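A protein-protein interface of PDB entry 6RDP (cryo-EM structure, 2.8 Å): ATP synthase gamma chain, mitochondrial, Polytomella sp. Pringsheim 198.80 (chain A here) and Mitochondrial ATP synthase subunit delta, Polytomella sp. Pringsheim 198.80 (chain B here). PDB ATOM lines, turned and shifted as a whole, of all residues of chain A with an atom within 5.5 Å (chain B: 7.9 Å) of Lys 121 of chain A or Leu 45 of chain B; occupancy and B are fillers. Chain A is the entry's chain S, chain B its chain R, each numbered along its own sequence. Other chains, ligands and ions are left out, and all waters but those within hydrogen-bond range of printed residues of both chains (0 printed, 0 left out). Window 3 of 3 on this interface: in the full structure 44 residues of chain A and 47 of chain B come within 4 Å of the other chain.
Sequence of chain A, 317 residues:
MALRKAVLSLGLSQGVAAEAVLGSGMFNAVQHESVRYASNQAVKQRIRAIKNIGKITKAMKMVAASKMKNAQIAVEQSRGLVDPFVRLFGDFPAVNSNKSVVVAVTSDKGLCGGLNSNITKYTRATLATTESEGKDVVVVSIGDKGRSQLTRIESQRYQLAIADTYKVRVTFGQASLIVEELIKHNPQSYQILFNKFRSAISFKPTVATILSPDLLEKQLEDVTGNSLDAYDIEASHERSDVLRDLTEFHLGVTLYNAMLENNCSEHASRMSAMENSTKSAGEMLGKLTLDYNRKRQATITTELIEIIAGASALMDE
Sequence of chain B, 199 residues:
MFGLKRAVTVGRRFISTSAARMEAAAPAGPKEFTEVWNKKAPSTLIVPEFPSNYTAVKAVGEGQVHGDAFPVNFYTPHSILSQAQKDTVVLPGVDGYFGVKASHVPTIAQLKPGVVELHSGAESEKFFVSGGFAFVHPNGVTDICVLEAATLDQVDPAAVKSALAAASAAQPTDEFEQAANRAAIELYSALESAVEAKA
The indole nitrogen (NE1) of Trp 37 of chain B is in hydrogen-bond range of the backbone carbonyl oxygen (O) of Ala 125 of chain A, at 2.6 Å. The side-chain hydroxyl (OH) of Tyr 122 of chain A lies within hydrogen-bond range of the backbone carbonyl oxygen (O) of Ile 46 of chain B (2.6 Å).
The side-chain hydroxyl (OG1) of Thr 126 of chain A sits at hydrogen-bond distance from the backbone carbonyl oxygen (O) of Tyr 122 of chain A (2.7 Å). The backbone carbonyl oxygen (O) of Thr 123 of chain A lies within hydrogen-bond range of the side-chain hydroxyl (OG1) of Thr 126 of chain A (3.3 Å).
Of the 11 printed residues of chain A, 4 touch a printed residue of chain B.
Of the printed residues of chain B, Lys 121 of chain A touches Leu 45 (3.9 Å). Leu 45 of chain B touches just these residues of chain A: Lys 121, Tyr 122 and Ala 125. Of the printed residues of chain B, Ala 125 of chain A touches Trp 37 (2.6 Å), Ala 41 (3.9 Å) and Leu 45 (3.9 Å). Printed residues of chain A within 4 Å of Trp 37 of chain B: Tyr 122 (3.7 Å), Ala 125 (2.6 Å) and Thr 126 (3.6 Å). Printed residues of chain B within 4 Å of Thr 126 of chain A: Trp 37 (3.6 Å) and Pro 48 (3.8 Å). Printed residues of chain A within 4 Å of Ala 41 of chain B: Ala 125. Thr 44 of chain B touches none of the printed residues of chain A. Pro 42 of chain B touches none of the printed residues of chain A. The nearest residue of chain B that does not touch Lys 121 of chain A is Trp 37 of chain B (6.5 Å). The nearest printed residue of chain A that does not touch Ala 41 of chain B is Thr 126 of chain A (5.8 Å).
Lys 121 of chain A touches Leu 45 of chain B. CH2 of Trp 37 of chain B touches CE1 of Tyr 122 of chain A, 3.7 Å away. CB of Leu 45 of chain B touches CE1 of Tyr 122 of chain A (3.6 Å). Ala 41 of chain B touches Ala 125 of chain A (CB to CB, 3.9 Å). CB of Ala 125 of chain A touches CD1 of Leu 45 of chain B (3.9 Å). Thr 126 of chain A touches Trp 37 of chain B (N to NE1, 3.6 Å). CG2 of Thr 126 of chain A touches CG of Pro 48 of chain B, at 3.8 Å.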
ATOM      1  N   ASN A 116     -12.432 -16.498 -21.377  1.00  0.00           N
ATOM      2  CA  ASN A 116     -13.130 -17.417 -22.255  1.00  0.00           C
ATOM      3  C   ASN A 116     -14.421 -17.934 -21.647  1.00  0.00           C
ATOM      4  O   ASN A 116     -15.375 -18.177 -22.381  1.00  0.00           O
ATOM      5  CB  ASN A 116     -12.218 -18.587 -22.586  1.00  0.00           C
ATOM      6  CG  ASN A 116     -10.856 -18.135 -23.018  1.00  0.00           C
ATOM      7  OD1 ASN A 116     -10.719 -17.172 -23.759  1.00  0.00           O
ATOM      8  ND2 ASN A 116      -9.831 -18.819 -22.542  1.00  0.00           N
ATOM      9  N   SER A 117     -14.486 -18.091 -20.327  1.00  0.00           N
ATOM     10  CA  SER A 117     -15.733 -18.509 -19.700  1.00  0.00           C
ATOM     11  C   SER A 117     -16.771 -17.407 -19.710  1.00  0.00           C
ATOM     12  O   SER A 117     -17.962 -17.691 -19.877  1.00  0.00           O
ATOM     13  CB  SER A 117     -15.488 -18.955 -18.261  1.00  0.00           C
ATOM     14  OG  SER A 117     -15.144 -17.856 -17.443  1.00  0.00           O
ATOM     15  N   ASN A 118     -16.339 -16.156 -19.545  1.00  0.00           N
ATOM     16  CA  ASN A 118     -17.240 -15.023 -19.692  1.00  0.00           C
ATOM     17  C   ASN A 118     -17.780 -14.931 -21.112  1.00  0.00           C
ATOM     18  O   ASN A 118     -18.963 -14.636 -21.317  1.00  0.00           O
ATOM     19  CB  ASN A 118     -16.506 -13.743 -19.306  1.00  0.00           C
ATOM     20  CG  ASN A 118     -17.401 -12.536 -19.286  1.00  0.00           C
ATOM     21  OD1 ASN A 118     -18.614 -12.646 -19.139  1.00  0.00           O
ATOM     22  ND2 ASN A 118     -16.802 -11.361 -19.421  1.00  0.00           N
ATOM     23  N   ILE A 119     -16.938 -15.218 -22.108  1.00  0.00           N
ATOM     24  CA  ILE A 119     -17.436 -15.278 -23.480  1.00  0.00           C
ATOM     25  C   ILE A 119     -18.338 -16.482 -23.710  1.00  0.00           C
ATOM     26  O   ILE A 119     -19.316 -16.377 -24.455  1.00  0.00           O
ATOM     27  CB  ILE A 119     -16.248 -15.236 -24.456  1.00  0.00           C
ATOM     28  CG1 ILE A 119     -15.548 -13.903 -24.300  1.00  0.00           C
ATOM     29  CG2 ILE A 119     -16.658 -15.392 -25.905  1.00  0.00           C
ATOM     30  CD1 ILE A 119     -16.431 -12.724 -24.645  1.00  0.00           C
ATOM     31  N   THR A 120     -18.084 -17.604 -23.040  1.00  0.00           N
ATOM     32  CA  THR A 120     -18.939 -18.773 -23.201  1.00  0.00           C
ATOM     33  C   THR A 120     -20.309 -18.531 -22.570  1.00  0.00           C
ATOM     34  O   THR A 120     -21.322 -19.046 -23.054  1.00  0.00           O
ATOM     35  CB  THR A 120     -18.251 -19.994 -22.594  1.00  0.00           C
ATOM     36  OG1 THR A 120     -16.937 -20.116 -23.139  1.00  0.00           O
ATOM     37  CG2 THR A 120     -19.002 -21.267 -22.920  1.00  0.00           C
ATOM     38  N   LYS A 121     -20.366 -17.717 -21.515  1.00  0.00           N
ATOM     39  CA  LYS A 121     -21.672 -17.410 -20.947  1.00  0.00           C
ATOM     40  C   LYS A 121     -22.387 -16.313 -21.734  1.00  0.00           C
ATOM     41  O   LYS A 121     -23.613 -16.372 -21.886  1.00  0.00           O
ATOM     42  CB  LYS A 121     -21.556 -17.055 -19.451  1.00  0.00           C
ATOM     43  CG  LYS A 121     -21.092 -15.655 -19.093  1.00  0.00           C
ATOM     44  CD  LYS A 121     -21.186 -15.372 -17.613  1.00  0.00           C
ATOM     45  CE  LYS A 121     -20.033 -15.995 -16.851  1.00  0.00           C
ATOM     46  NZ  LYS A 121     -20.022 -15.551 -15.428  1.00  0.00           N
ATOM     47  N   TYR A 122     -21.662 -15.335 -22.295  1.00  0.00           N
ATOM     48  CA  TYR A 122     -22.329 -14.365 -23.158  1.00  0.00           C
ATOM     49  C   TYR A 122     -22.720 -14.969 -24.496  1.00  0.00           C
ATOM     50  O   TYR A 122     -23.597 -14.423 -25.171  1.00  0.00           O
ATOM     51  CB  TYR A 122     -21.473 -13.129 -23.390  1.00  0.00           C
ATOM     52  CG  TYR A 122     -21.627 -12.049 -22.356  1.00  0.00           C
ATOM     53  CD1 TYR A 122     -22.638 -12.093 -21.423  1.00  0.00           C
ATOM     54  CD2 TYR A 122     -20.796 -10.947 -22.363  1.00  0.00           C
ATOM     55  CE1 TYR A 122     -22.785 -11.084 -20.491  1.00  0.00           C
ATOM     56  CE2 TYR A 122     -20.931  -9.940 -21.442  1.00  0.00           C
ATOM     57  CZ  TYR A 122     -21.928 -10.008 -20.509  1.00  0.00           C
ATOM     58  OH  TYR A 122     -22.064  -8.995 -19.591  1.00  0.00           O
ATOM     59  N   THR A 123     -22.096 -16.086 -24.879  1.00  0.00           N
ATOM     60  CA  THR A 123     -22.526 -16.840 -26.047  1.00  0.00           C
ATOM     61  C   THR A 123     -23.970 -17.283 -25.902  1.00  0.00           C
ATOM     62  O   THR A 123     -24.810 -16.965 -26.746  1.00  0.00           O
ATOM     63  CB  THR A 123     -21.612 -18.043 -26.252  1.00  0.00           C
ATOM     64  OG1 THR A 123     -20.349 -17.589 -26.738  1.00  0.00           O
ATOM     65  CG2 THR A 123     -22.204 -19.021 -27.253  1.00  0.00           C
ATOM     66  N   ARG A 124     -24.298 -17.952 -24.795  1.00  0.00           N
ATOM     67  CA  ARG A 124     -25.681 -18.368 -24.597  1.00  0.00           C
ATOM     68  C   ARG A 124     -26.577 -17.194 -24.207  1.00  0.00           C
ATOM     69  O   ARG A 124     -27.765 -17.198 -24.550  1.00  0.00           O
ATOM     70  CB  ARG A 124     -25.750 -19.489 -23.561  1.00  0.00           C
ATOM     71  CG  ARG A 124     -25.400 -19.089 -22.147  1.00  0.00           C
ATOM     72  CD  ARG A 124     -25.050 -20.289 -21.303  1.00  0.00           C
ATOM     73  NE  ARG A 124     -26.177 -21.202 -21.156  1.00  0.00           N
ATOM     74  CZ  ARG A 124     -27.112 -21.096 -20.221  1.00  0.00           C
ATOM     75  NH1 ARG A 124     -27.063 -20.115 -19.333  1.00  0.00           N
ATOM     76  NH2 ARG A 124     -28.099 -21.978 -20.175  1.00  0.00           N
ATOM     77  N   ALA A 125     -26.021 -16.157 -23.561  1.00  0.00           N
ATOM     78  CA  ALA A 125     -26.825 -15.000 -23.166  1.00  0.00           C
ATOM     79  C   ALA A 125     -27.281 -14.179 -24.362  1.00  0.00           C
ATOM     80  O   ALA A 125     -28.365 -13.586 -24.328  1.00  0.00           O
ATOM     81  CB  ALA A 125     -26.041 -14.114 -22.207  1.00  0.00           C
ATOM     82  N   THR A 126     -26.466 -14.113 -25.412  1.00  0.00           N
ATOM     83  CA  THR A 126     -26.868 -13.479 -26.655  1.00  0.00           C
ATOM     84  C   THR A 126     -27.460 -14.461 -27.655  1.00  0.00           C
ATOM     85  O   THR A 126     -28.060 -14.023 -28.639  1.00  0.00           O
ATOM     86  CB  THR A 126     -25.677 -12.769 -27.301  1.00  0.00           C
ATOM     87  OG1 THR A 126     -24.640 -13.722 -27.544  1.00  0.00           O
ATOM     88  CG2 THR A 126     -25.146 -11.679 -26.387  1.00  0.00           C
ATOM     89  N   TRP B  37     -32.765  -8.125 -24.221  1.00  0.00           N
ATOM     90  CA  TRP B  37     -31.726  -8.917 -23.575  1.00  0.00           C
ATOM     91  C   TRP B  37     -31.830  -8.898 -22.053  1.00  0.00           C
ATOM     92  O   TRP B  37     -31.246  -9.763 -21.393  1.00  0.00           O
ATOM     93  CB  TRP B  37     -30.360  -8.409 -24.032  1.00  0.00           C
ATOM     94  CG  TRP B  37     -29.234  -9.343 -23.774  1.00  0.00           C
ATOM     95  CD1 TRP B  37     -28.920 -10.459 -24.483  1.00  0.00           C
ATOM     96  CD2 TRP B  37     -28.243  -9.223 -22.758  1.00  0.00           C
ATOM     97  NE1 TRP B  37     -27.809 -11.060 -23.957  1.00  0.00           N
ATOM     98  CE2 TRP B  37     -27.371 -10.316 -22.896  1.00  0.00           C
ATOM     99  CE3 TRP B  37     -28.013  -8.301 -21.738  1.00  0.00           C
ATOM    100  CZ2 TRP B  37     -26.292 -10.507 -22.061  1.00  0.00           C
ATOM    101  CZ3 TRP B  37     -26.954  -8.505 -20.908  1.00  0.00           C
ATOM    102  CH2 TRP B  37     -26.098  -9.588 -21.078  1.00  0.00           C
ATOM    103  N   ASN B  38     -32.575  -7.952 -21.484  1.00  0.00           N
ATOM    104  CA  ASN B  38     -32.865  -7.953 -20.055  1.00  0.00           C
ATOM    105  C   ASN B  38     -34.010  -8.884 -19.681  1.00  0.00           C
ATOM    106  O   ASN B  38     -34.461  -8.849 -18.532  1.00  0.00           O
ATOM    107  CB  ASN B  38     -33.195  -6.541 -19.564  1.00  0.00           C
ATOM    108  CG  ASN B  38     -32.039  -5.574 -19.721  1.00  0.00           C
ATOM    109  OD1 ASN B  38     -32.228  -4.362 -19.655  1.00  0.00           O
ATOM    110  ND2 ASN B  38     -30.835  -6.103 -19.903  1.00  0.00           N
ATOM    111  N   LYS B  40     -34.186 -12.417 -21.250  1.00  0.00           N
ATOM    112  CA  LYS B  40     -33.794 -13.804 -21.455  1.00  0.00           C
ATOM    113  C   LYS B  40     -32.444 -14.155 -20.840  1.00  0.00           C
ATOM    114  O   LYS B  40     -32.245 -15.297 -20.423  1.00  0.00           O
ATOM    115  CB  LYS B  40     -33.764 -14.122 -22.954  1.00  0.00           C
ATOM    116  CG  LYS B  40     -33.793 -15.597 -23.267  1.00  0.00           C
ATOM    117  CD  LYS B  40     -35.125 -16.200 -22.909  1.00  0.00           C
ATOM    118  CE  LYS B  40     -36.187 -15.707 -23.862  1.00  0.00           C
ATOM    119  NZ  LYS B  40     -35.926 -16.194 -25.248  1.00  0.00           N
ATOM    120  N   ALA B  41     -31.517 -13.212 -20.780  1.00  0.00           N
ATOM    121  CA  ALA B  41     -30.279 -13.417 -20.052  1.00  0.00           C
ATOM    122  C   ALA B  41     -30.520 -13.213 -18.560  1.00  0.00           C
ATOM    123  O   ALA B  41     -31.525 -12.614 -18.165  1.00  0.00           O
ATOM    124  CB  ALA B  41     -29.213 -12.452 -20.559  1.00  0.00           C
ATOM    125  N   PRO B  42     -29.639 -13.740 -17.702  1.00  0.00           N
ATOM    126  CA  PRO B  42     -29.705 -13.376 -16.280  1.00  0.00           C
ATOM    127  C   PRO B  42     -29.402 -11.897 -16.087  1.00  0.00           C
ATOM    128  O   PRO B  42     -28.587 -11.314 -16.801  1.00  0.00           O
ATOM    129  CB  PRO B  42     -28.643 -14.268 -15.628  1.00  0.00           C
ATOM    130  CG  PRO B  42     -27.846 -14.838 -16.759  1.00  0.00           C
ATOM    131  CD  PRO B  42     -28.776 -14.913 -17.914  1.00  0.00           C
ATOM    132  N   SER B  43     -30.083 -11.294 -15.112  1.00  0.00           N
ATOM    133  CA  SER B  43     -30.156  -9.844 -14.997  1.00  0.00           C
ATOM    134  C   SER B  43     -28.864  -9.196 -14.521  1.00  0.00           C
ATOM    135  O   SER B  43     -28.691  -7.989 -14.721  1.00  0.00           O
ATOM    136  CB  SER B  43     -31.296  -9.453 -14.051  1.00  0.00           C
ATOM    137  OG  SER B  43     -30.985  -9.796 -12.715  1.00  0.00           O
ATOM    138  N   THR B  44     -27.952  -9.951 -13.910  1.00  0.00           N
ATOM    139  CA  THR B  44     -26.716  -9.362 -13.412  1.00  0.00           C
ATOM    140  C   THR B  44     -25.724  -9.079 -14.537  1.00  0.00           C
ATOM    141  O   THR B  44     -24.830  -8.240 -14.371  1.00  0.00           O
ATOM    142  CB  THR B  44     -26.098 -10.293 -12.361  1.00  0.00           C
ATOM    143  OG1 THR B  44     -27.142 -10.823 -11.535  1.00  0.00           O
ATOM    144  CG2 THR B  44     -25.123  -9.546 -11.458  1.00  0.00           C
ATOM    145  N   LEU B  45     -25.891  -9.722 -15.688  1.00  0.00           N
ATOM    146  CA  LEU B  45     -25.001  -9.506 -16.820  1.00  0.00           C
ATOM    147  C   LEU B  45     -25.258  -8.145 -17.461  1.00  0.00           C
ATOM    148  O   LEU B  45     -26.384  -7.833 -17.852  1.00  0.00           O
ATOM    149  CB  LEU B  45     -25.185 -10.615 -17.851  1.00  0.00           C
ATOM    150  CG  LEU B  45     -24.818 -12.037 -17.434  1.00  0.00           C
ATOM    151  CD1 LEU B  45     -25.140 -13.021 -18.549  1.00  0.00           C
ATOM    152  CD2 LEU B  45     -23.352 -12.125 -17.037  1.00  0.00           C
ATOM    153  N   ILE B  46     -24.205  -7.332 -17.543  1.00  0.00           N
ATOM    154  CA  ILE B  46     -24.274  -6.052 -18.232  1.00  0.00           C
ATOM    155  C   ILE B  46     -24.438  -6.324 -19.728  1.00  0.00           C
ATOM    156  O   ILE B  46     -24.005  -7.369 -20.232  1.00  0.00           O
ATOM    157  CB  ILE B  46     -23.012  -5.214 -17.926  1.00  0.00           C
ATOM    158  CG1 ILE B  46     -22.794  -5.051 -16.414  1.00  0.00           C
ATOM    159  CG2 ILE B  46     -23.089  -3.796 -18.472  1.00  0.00           C
ATOM    160  CD1 ILE B  46     -21.738  -5.970 -15.799  1.00  0.00           C
ATOM    161  N   VAL B  47     -25.113  -5.409 -20.425  1.00  0.00           N
ATOM    162  CA  VAL B  47     -25.379  -5.512 -21.868  1.00  0.00           C
ATOM    163  C   VAL B  47     -24.064  -5.623 -22.637  1.00  0.00           C
ATOM    164  O   VAL B  47     -23.091  -4.911 -22.315  1.00  0.00           O
ATOM    165  CB  VAL B  47     -26.233  -4.312 -22.343  1.00  0.00           C
ATOM    166  CG1 VAL B  47     -25.616  -2.973 -21.941  1.00  0.00           C
ATOM    167  CG2 VAL B  47     -26.461  -4.357 -23.846  1.00  0.00           C
ATOM    168  N   PRO B  48     -23.938  -6.574 -23.568  1.00  0.00           N
ATOM    169  CA  PRO B  48     -22.729  -6.643 -24.388  1.00  0.00           C
ATOM    170  C   PRO B  48     -22.625  -5.415 -25.266  1.00  0.00           C
ATOM    171  O   PRO B  48     -23.630  -4.888 -25.742  1.00  0.00           O
ATOM    172  CB  PRO B  48     -22.933  -7.916 -25.216  1.00  0.00           C
ATOM    173  CG  PRO B  48     -24.377  -8.146 -25.211  1.00  0.00           C
ATOM    174  CD  PRO B  48     -24.865  -7.673 -23.884  1.00  0.00           C
